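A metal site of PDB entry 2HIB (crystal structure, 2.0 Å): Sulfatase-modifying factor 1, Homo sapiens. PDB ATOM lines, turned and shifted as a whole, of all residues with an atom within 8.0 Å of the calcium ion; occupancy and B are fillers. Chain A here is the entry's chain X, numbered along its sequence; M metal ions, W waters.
The guanidinium group of Arg 279 sits close to the backbone carbonyl oxygen of Asn 208 (3.5 Å). ND2 of Asn 212 sits at hydrogen-bond distance from OE1 of Glu 45 (2.9 Å). O of Gly 246 sits at hydrogen-bond distance from N of Gly 211 (2.9 Å). OE1 of Glu 215 is in salt-bridge range of NE of Arg 279 (2.8 Å). The backbone carbonyl oxygen (O) of Glu 215 lies within hydrogen-bond range of the backbone NH (N) of Lys 245, at 2.8 Å. The indole nitrogen of Trp 146 sits at hydrogen-bond distance from the side-chain carboxylate of Glu 215, at 2.9 Å.
The calcium ion is bound by water W1 (2.2 Å), the backbone carbonyl oxygen of Asn 208 (2.4 Å), the side-chain carboxylate of Glu 45 (2.4 Å), the backbone carbonyl oxygen of Ala 213 (2.4 Å), the backbone carbonyl oxygen of Gly 211 (2.4 Å) and the side-chain carboxylate of Glu 215 (2.4 Å).
Residues that only touch the calcium ion: Ile 209 (3.7 Å). Six residues have an atom within 4 Å of the calcium ion: Glu 45, Asn 208, Ile 209, Gly 211, Ala 213 and Glu 215. The nearest printed residue that does not touch the calcium ion is Val 210 (4.3 Å).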
ATOM      1  N   TYR A  44     -22.247  17.617 -12.499  1.00  0.00           N
ATOM      2  CA  TYR A  44     -22.186  16.710 -11.377  1.00  0.00           C
ATOM      3  C   TYR A  44     -21.370  15.456 -11.673  1.00  0.00           C
ATOM      4  O   TYR A  44     -21.329  14.967 -12.820  1.00  0.00           O
ATOM      5  CB  TYR A  44     -23.588  16.227 -11.021  1.00  0.00           C
ATOM      6  CG  TYR A  44     -24.595  17.319 -10.880  1.00  0.00           C
ATOM      7  CD1 TYR A  44     -24.557  18.200  -9.829  1.00  0.00           C
ATOM      8  CD2 TYR A  44     -25.596  17.465 -11.817  1.00  0.00           C
ATOM      9  CE1 TYR A  44     -25.482  19.211  -9.699  1.00  0.00           C
ATOM     10  CE2 TYR A  44     -26.532  18.476 -11.702  1.00  0.00           C
ATOM     11  CZ  TYR A  44     -26.474  19.348 -10.656  1.00  0.00           C
ATOM     12  OH  TYR A  44     -27.408  20.372 -10.569  1.00  0.00           O
ATOM     13  N   GLU A  45     -20.768  14.929 -10.615  1.00  0.00           N
ATOM     14  CA  GLU A  45     -20.281  13.557 -10.611  1.00  0.00           C
ATOM     15  C   GLU A  45     -21.417  12.644 -11.049  1.00  0.00           C
ATOM     16  O   GLU A  45     -22.587  12.900 -10.739  1.00  0.00           O
ATOM     17  CB  GLU A  45     -19.800  13.144  -9.232  1.00  0.00           C
ATOM     18  CG  GLU A  45     -18.537  13.865  -8.764  1.00  0.00           C
ATOM     19  CD  GLU A  45     -18.465  13.985  -7.247  1.00  0.00           C
ATOM     20  OE1 GLU A  45     -19.525  14.092  -6.611  1.00  0.00           O
ATOM     21  OE2 GLU A  45     -17.340  13.999  -6.692  1.00  0.00           O
ATOM     22  N   PRO A 120     -22.494  10.071  -5.619  1.00  0.00           N
ATOM     23  CA  PRO A 120     -21.689   9.645  -6.766  1.00  0.00           C
ATOM     24  C   PRO A 120     -21.478   8.156  -6.792  1.00  0.00           C
ATOM     25  O   PRO A 120     -21.311   7.539  -5.732  1.00  0.00           O
ATOM     26  CB  PRO A 120     -20.346  10.352  -6.544  1.00  0.00           C
ATOM     27  CG  PRO A 120     -20.311  10.653  -5.099  1.00  0.00           C
ATOM     28  CD  PRO A 120     -21.709  10.871  -4.674  1.00  0.00           C
ATOM     29  N   TRP A 146     -10.227  19.009 -17.352  1.00  0.00           N
ATOM     30  CA  TRP A 146     -10.684  18.831 -16.008  1.00  0.00           C
ATOM     31  C   TRP A 146     -10.167  19.988 -15.136  1.00  0.00           C
ATOM     32  O   TRP A 146     -10.950  20.635 -14.438  1.00  0.00           O
ATOM     33  CB  TRP A 146     -10.221  17.465 -15.445  1.00  0.00           C
ATOM     34  CG  TRP A 146     -10.855  17.147 -14.181  1.00  0.00           C
ATOM     35  CD1 TRP A 146     -11.924  16.332 -13.979  1.00  0.00           C
ATOM     36  CD2 TRP A 146     -10.528  17.690 -12.901  1.00  0.00           C
ATOM     37  NE1 TRP A 146     -12.252  16.293 -12.655  1.00  0.00           N
ATOM     38  CE2 TRP A 146     -11.419  17.140 -11.974  1.00  0.00           C
ATOM     39  CE3 TRP A 146      -9.538  18.565 -12.447  1.00  0.00           C
ATOM     40  CZ2 TRP A 146     -11.364  17.441 -10.621  1.00  0.00           C
ATOM     41  CZ3 TRP A 146      -9.493  18.865 -11.136  1.00  0.00           C
ATOM     42  CH2 TRP A 146     -10.405  18.311 -10.216  1.00  0.00           C
ATOM     43  N   ASN A 174     -16.763  18.639   0.237  1.00  0.00           N
ATOM     44  CA  ASN A 174     -16.803  17.470   1.108  1.00  0.00           C
ATOM     45  C   ASN A 174     -15.402  16.817   1.198  1.00  0.00           C
ATOM     46  O   ASN A 174     -15.007  16.033   0.342  1.00  0.00           O
ATOM     47  CB  ASN A 174     -17.856  16.480   0.638  1.00  0.00           C
ATOM     48  CG  ASN A 174     -17.999  15.298   1.595  1.00  0.00           C
ATOM     49  OD1 ASN A 174     -17.527  15.368   2.733  1.00  0.00           O
ATOM     50  ND2 ASN A 174     -18.591  14.210   1.130  1.00  0.00           N
ATOM     51  N   TYR A 207     -20.249  21.232  -9.619  1.00  0.00           N
ATOM     52  CA  TYR A 207     -20.388  20.853  -8.216  1.00  0.00           C
ATOM     53  C   TYR A 207     -19.396  19.763  -7.854  1.00  0.00           C
ATOM     54  O   TYR A 207     -19.182  18.820  -8.619  1.00  0.00           O
ATOM     55  CB  TYR A 207     -21.809  20.376  -7.939  1.00  0.00           C
ATOM     56  CG  TYR A 207     -22.844  21.458  -8.109  1.00  0.00           C
ATOM     57  CD1 TYR A 207     -23.289  21.851  -9.366  1.00  0.00           C
ATOM     58  CD2 TYR A 207     -23.366  22.126  -7.008  1.00  0.00           C
ATOM     59  CE1 TYR A 207     -24.226  22.830  -9.511  1.00  0.00           C
ATOM     60  CE2 TYR A 207     -24.312  23.113  -7.146  1.00  0.00           C
ATOM     61  CZ  TYR A 207     -24.719  23.486  -8.416  1.00  0.00           C
ATOM     62  OH  TYR A 207     -25.667  24.459  -8.553  1.00  0.00           O
ATOM     63  N   ASN A 208     -18.785  19.895  -6.697  1.00  0.00           N
ATOM     64  CA  ASN A 208     -17.960  18.857  -6.104  1.00  0.00           C
ATOM     65  C   ASN A 208     -16.808  18.414  -6.980  1.00  0.00           C
ATOM     66  O   ASN A 208     -16.416  17.253  -6.985  1.00  0.00           O
ATOM     67  CB  ASN A 208     -18.826  17.656  -5.659  1.00  0.00           C
ATOM     68  CG  ASN A 208     -19.865  18.048  -4.625  1.00  0.00           C
ATOM     69  OD1 ASN A 208     -19.539  18.414  -3.479  1.00  0.00           O
ATOM     70  ND2 ASN A 208     -21.147  18.002  -5.038  1.00  0.00           N
ATOM     71  N   ILE A 209     -16.262  19.363  -7.734  1.00  0.00           N
ATOM     72  CA  ILE A 209     -15.129  19.095  -8.589  1.00  0.00           C
ATOM     73  C   ILE A 209     -13.872  18.807  -7.723  1.00  0.00           C
ATOM     74  O   ILE A 209     -13.079  17.932  -8.072  1.00  0.00           O
ATOM     75  CB  ILE A 209     -14.943  20.210  -9.642  1.00  0.00           C
ATOM     76  CG1 ILE A 209     -13.948  19.785 -10.724  1.00  0.00           C
ATOM     77  CG2 ILE A 209     -14.534  21.543  -8.990  1.00  0.00           C
ATOM     78  CD1 ILE A 209     -14.524  18.870 -11.762  1.00  0.00           C
ATOM     79  N   VAL A 210     -13.729  19.480  -6.577  1.00  0.00           N
ATOM     80  CA  VAL A 210     -12.820  19.000  -5.534  1.00  0.00           C
ATOM     81  C   VAL A 210     -13.664  18.360  -4.398  1.00  0.00           C
ATOM     82  O   VAL A 210     -14.792  18.790  -4.102  1.00  0.00           O
ATOM     83  CB  VAL A 210     -11.817  20.070  -4.982  1.00  0.00           C
ATOM     84  CG1 VAL A 210     -10.840  20.566  -6.083  1.00  0.00           C
ATOM     85  CG2 VAL A 210     -12.557  21.238  -4.306  1.00  0.00           C
ATOM     86  N   GLY A 211     -13.099  17.334  -3.785  1.00  0.00           N
ATOM     87  CA  GLY A 211     -13.759  16.625  -2.730  1.00  0.00           C
ATOM     88  C   GLY A 211     -14.847  15.683  -3.217  1.00  0.00           C
ATOM     89  O   GLY A 211     -15.050  15.505  -4.434  1.00  0.00           O
ATOM     90  N   ASN A 212     -15.532  15.095  -2.245  1.00  0.00           N
ATOM     91  CA  ASN A 212     -16.558  14.099  -2.475  1.00  0.00           C
ATOM     92  C   ASN A 212     -15.976  12.805  -3.054  1.00  0.00           C
ATOM     93  O   ASN A 212     -15.434  12.015  -2.282  1.00  0.00           O
ATOM     94  CB  ASN A 212     -17.751  14.674  -3.275  1.00  0.00           C
ATOM     95  CG  ASN A 212     -19.086  14.087  -2.830  1.00  0.00           C
ATOM     96  OD1 ASN A 212     -19.228  13.661  -1.687  1.00  0.00           O
ATOM     97  ND2 ASN A 212     -20.094  14.100  -3.726  1.00  0.00           N
ATOM     98  N   ALA A 213     -16.053  12.573  -4.360  1.00  0.00           N
ATOM     99  CA  ALA A 213     -15.340  11.438  -4.995  1.00  0.00           C
ATOM    100  C   ALA A 213     -14.180  11.965  -5.856  1.00  0.00           C
ATOM    101  O   ALA A 213     -14.287  13.028  -6.476  1.00  0.00           O
ATOM    102  CB  ALA A 213     -16.293  10.592  -5.840  1.00  0.00           C
ATOM    103  N   TRP A 214     -13.062  11.222  -5.856  1.00  0.00           N
ATOM    104  CA  TRP A 214     -12.034  11.402  -6.872  1.00  0.00           C
ATOM    105  C   TRP A 214     -12.653  11.262  -8.255  1.00  0.00           C
ATOM    106  O   TRP A 214     -13.681  10.589  -8.421  1.00  0.00           O
ATOM    107  CB  TRP A 214     -10.933  10.359  -6.767  1.00  0.00           C
ATOM    108  CG  TRP A 214      -9.872  10.620  -5.790  1.00  0.00           C
ATOM    109  CD1 TRP A 214      -9.784  10.114  -4.530  1.00  0.00           C
ATOM    110  CD2 TRP A 214      -8.679  11.384  -6.011  1.00  0.00           C
ATOM    111  NE1 TRP A 214      -8.647  10.557  -3.922  1.00  0.00           N
ATOM    112  CE2 TRP A 214      -7.940  11.331  -4.817  1.00  0.00           C
ATOM    113  CE3 TRP A 214      -8.185  12.134  -7.075  1.00  0.00           C
ATOM    114  CZ2 TRP A 214      -6.722  11.994  -4.664  1.00  0.00           C
ATOM    115  CZ3 TRP A 214      -6.967  12.789  -6.929  1.00  0.00           C
ATOM    116  CH2 TRP A 214      -6.261  12.718  -5.741  1.00  0.00           C
ATOM    117  N   GLU A 215     -12.017  11.861  -9.249  1.00  0.00           N
ATOM    118  CA  GLU A 215     -12.537  11.803 -10.600  1.00  0.00           C
ATOM    119  C   GLU A 215     -11.501  11.381 -11.647  1.00  0.00           C
ATOM    120  O   GLU A 215     -10.444  12.023 -11.791  1.00  0.00           O
ATOM    121  CB  GLU A 215     -13.111  13.177 -10.952  1.00  0.00           C
ATOM    122  CG  GLU A 215     -14.159  13.578  -9.925  1.00  0.00           C
ATOM    123  CD  GLU A 215     -14.835  14.875 -10.196  1.00  0.00           C
ATOM    124  OE1 GLU A 215     -14.715  15.448 -11.303  1.00  0.00           O
ATOM    125  OE2 GLU A 215     -15.535  15.308  -9.262  1.00  0.00           O
ATOM    126  N   LYS A 245      -8.206  13.200 -10.532  1.00  0.00           N
ATOM    127  CA  LYS A 245      -8.116  14.545 -10.017  1.00  0.00           C
ATOM    128  C   LYS A 245      -9.139  14.831  -8.929  1.00  0.00           C
ATOM    129  O   LYS A 245     -10.194  14.200  -8.856  1.00  0.00           O
ATOM    130  CB  LYS A 245      -8.356  15.553 -11.137  1.00  0.00           C
ATOM    131  CG  LYS A 245      -7.394  15.514 -12.293  1.00  0.00           C
ATOM    132  CD  LYS A 245      -6.061  16.135 -11.961  1.00  0.00           C
ATOM    133  CE  LYS A 245      -6.038  17.625 -12.231  1.00  0.00           C
ATOM    134  NZ  LYS A 245      -4.691  18.200 -11.926  1.00  0.00           N
ATOM    135  N   GLY A 246      -8.790  15.843  -8.115  1.00  0.00           N
ATOM    136  CA  GLY A 246      -9.746  16.573  -7.293  1.00  0.00           C
ATOM    137  C   GLY A 246      -9.910  16.156  -5.846  1.00  0.00           C
ATOM    138  O   GLY A 246     -10.576  16.862  -5.079  1.00  0.00           O
ATOM    139  N   GLY A 247      -9.348  15.020  -5.441  1.00  0.00           N
ATOM    140  CA  GLY A 247      -9.480  14.611  -4.051  1.00  0.00           C
ATOM    141  C   GLY A 247     -10.870  14.061  -3.728  1.00  0.00           C
ATOM    142  O   GLY A 247     -11.715  13.927  -4.602  1.00  0.00           O
ATOM    143  N   SER A 248     -11.089  13.757  -2.455  1.00  0.00           N
ATOM    144  CA  SER A 248     -12.270  13.029  -2.024  1.00  0.00           C
ATOM    145  C   SER A 248     -12.648  13.421  -0.627  1.00  0.00           C
ATOM    146  O   SER A 248     -11.962  14.213   0.013  1.00  0.00           O
ATOM    147  CB  SER A 248     -11.991  11.519  -2.036  1.00  0.00           C
ATOM    148  OG  SER A 248     -11.350  11.085  -0.833  1.00  0.00           O
ATOM    149  N   TYR A 249     -13.725  12.804  -0.137  1.00  0.00           N
ATOM    150  CA  TYR A 249     -14.209  13.056   1.202  1.00  0.00           C
ATOM    151  C   TYR A 249     -13.183  12.627   2.279  1.00  0.00           C
ATOM    152  O   TYR A 249     -13.336  12.946   3.475  1.00  0.00           O
ATOM    153  CB  TYR A 249     -15.555  12.367   1.404  1.00  0.00           C
ATOM    154  CG  TYR A 249     -15.518  10.850   1.385  1.00  0.00           C
ATOM    155  CD1 TYR A 249     -15.110  10.149   2.507  1.00  0.00           C
ATOM    156  CD2 TYR A 249     -15.949  10.128   0.283  1.00  0.00           C
ATOM    157  CE1 TYR A 249     -15.099   8.758   2.532  1.00  0.00           C
ATOM    158  CE2 TYR A 249     -15.951   8.717   0.301  1.00  0.00           C
ATOM    159  CZ  TYR A 249     -15.526   8.064   1.428  1.00  0.00           C
ATOM    160  OH  TYR A 249     -15.513   6.696   1.487  1.00  0.00           O
ATOM    161  N   ASN A 275     -13.756   5.679  -2.745  1.00  0.00           N
ATOM    162  CA  ASN A 275     -13.639   7.130  -2.835  1.00  0.00           C
ATOM    163  C   ASN A 275     -13.381   7.650  -4.258  1.00  0.00           C
ATOM    164  O   ASN A 275     -12.979   8.793  -4.406  1.00  0.00           O
ATOM    165  CB  ASN A 275     -12.548   7.628  -1.898  1.00  0.00           C
ATOM    166  CG  ASN A 275     -11.148   7.265  -2.373  1.00  0.00           C
ATOM    167  OD1 ASN A 275     -10.962   6.489  -3.315  1.00  0.00           O
ATOM    168  ND2 ASN A 275     -10.155   7.855  -1.729  1.00  0.00           N
ATOM    169  N   GLY A 277     -14.696   8.065  -8.329  1.00  0.00           N
ATOM    170  CA  GLY A 277     -15.761   8.096  -9.311  1.00  0.00           C
ATOM    171  C   GLY A 277     -15.359   8.907 -10.534  1.00  0.00           C
ATOM    172  O   GLY A 277     -14.187   8.910 -10.948  1.00  0.00           O
ATOM    173  N   PHE A 278     -16.327   9.607 -11.113  1.00  0.00           N
ATOM    174  CA  PHE A 278     -16.052  10.362 -12.333  1.00  0.00           C
ATOM    175  C   PHE A 278     -17.178  11.260 -12.751  1.00  0.00           C
ATOM    176  O   PHE A 278     -18.293  11.161 -12.241  1.00  0.00           O
ATOM    177  CB  PHE A 278     -15.684   9.419 -13.487  1.00  0.00           C
ATOM    178  CG  PHE A 278     -16.830   8.576 -13.986  1.00  0.00           C
ATOM    179  CD1 PHE A 278     -17.293   7.481 -13.232  1.00  0.00           C
ATOM    180  CD2 PHE A 278     -17.457   8.886 -15.204  1.00  0.00           C
ATOM    181  CE1 PHE A 278     -18.352   6.700 -13.690  1.00  0.00           C
ATOM    182  CE2 PHE A 278     -18.505   8.110 -15.670  1.00  0.00           C
ATOM    183  CZ  PHE A 278     -18.958   7.007 -14.909  1.00  0.00           C
ATOM    184  N   ARG A 279     -16.870  12.144 -13.701  1.00  0.00           N
ATOM    185  CA  ARG A 279     -17.884  12.863 -14.458  1.00  0.00           C
ATOM    186  C   ARG A 279     -17.478  12.864 -15.943  1.00  0.00           C
ATOM    187  O   ARG A 279     -16.299  12.677 -16.271  1.00  0.00           O
ATOM    188  CB  ARG A 279     -18.008  14.277 -13.932  1.00  0.00           C
ATOM    189  CG  ARG A 279     -16.853  15.208 -14.372  1.00  0.00           C
ATOM    190  CD  ARG A 279     -17.046  16.629 -13.861  1.00  0.00           C
ATOM    191  NE  ARG A 279     -16.946  16.651 -12.404  1.00  0.00           N
ATOM    192  CZ  ARG A 279     -17.775  17.260 -11.555  1.00  0.00           C
ATOM    193  NH1 ARG A 279     -18.823  17.976 -11.979  1.00  0.00           N
ATOM    194  NH2 ARG A 279     -17.538  17.151 -10.254  1.00  0.00           N
HETATM  195 CA    CA M   1     -15.290  15.182  -6.835  1.00  0.00          CA
HETATM  196  O   HOH W   1     -13.112  15.603  -6.923  1.00  0.00           O
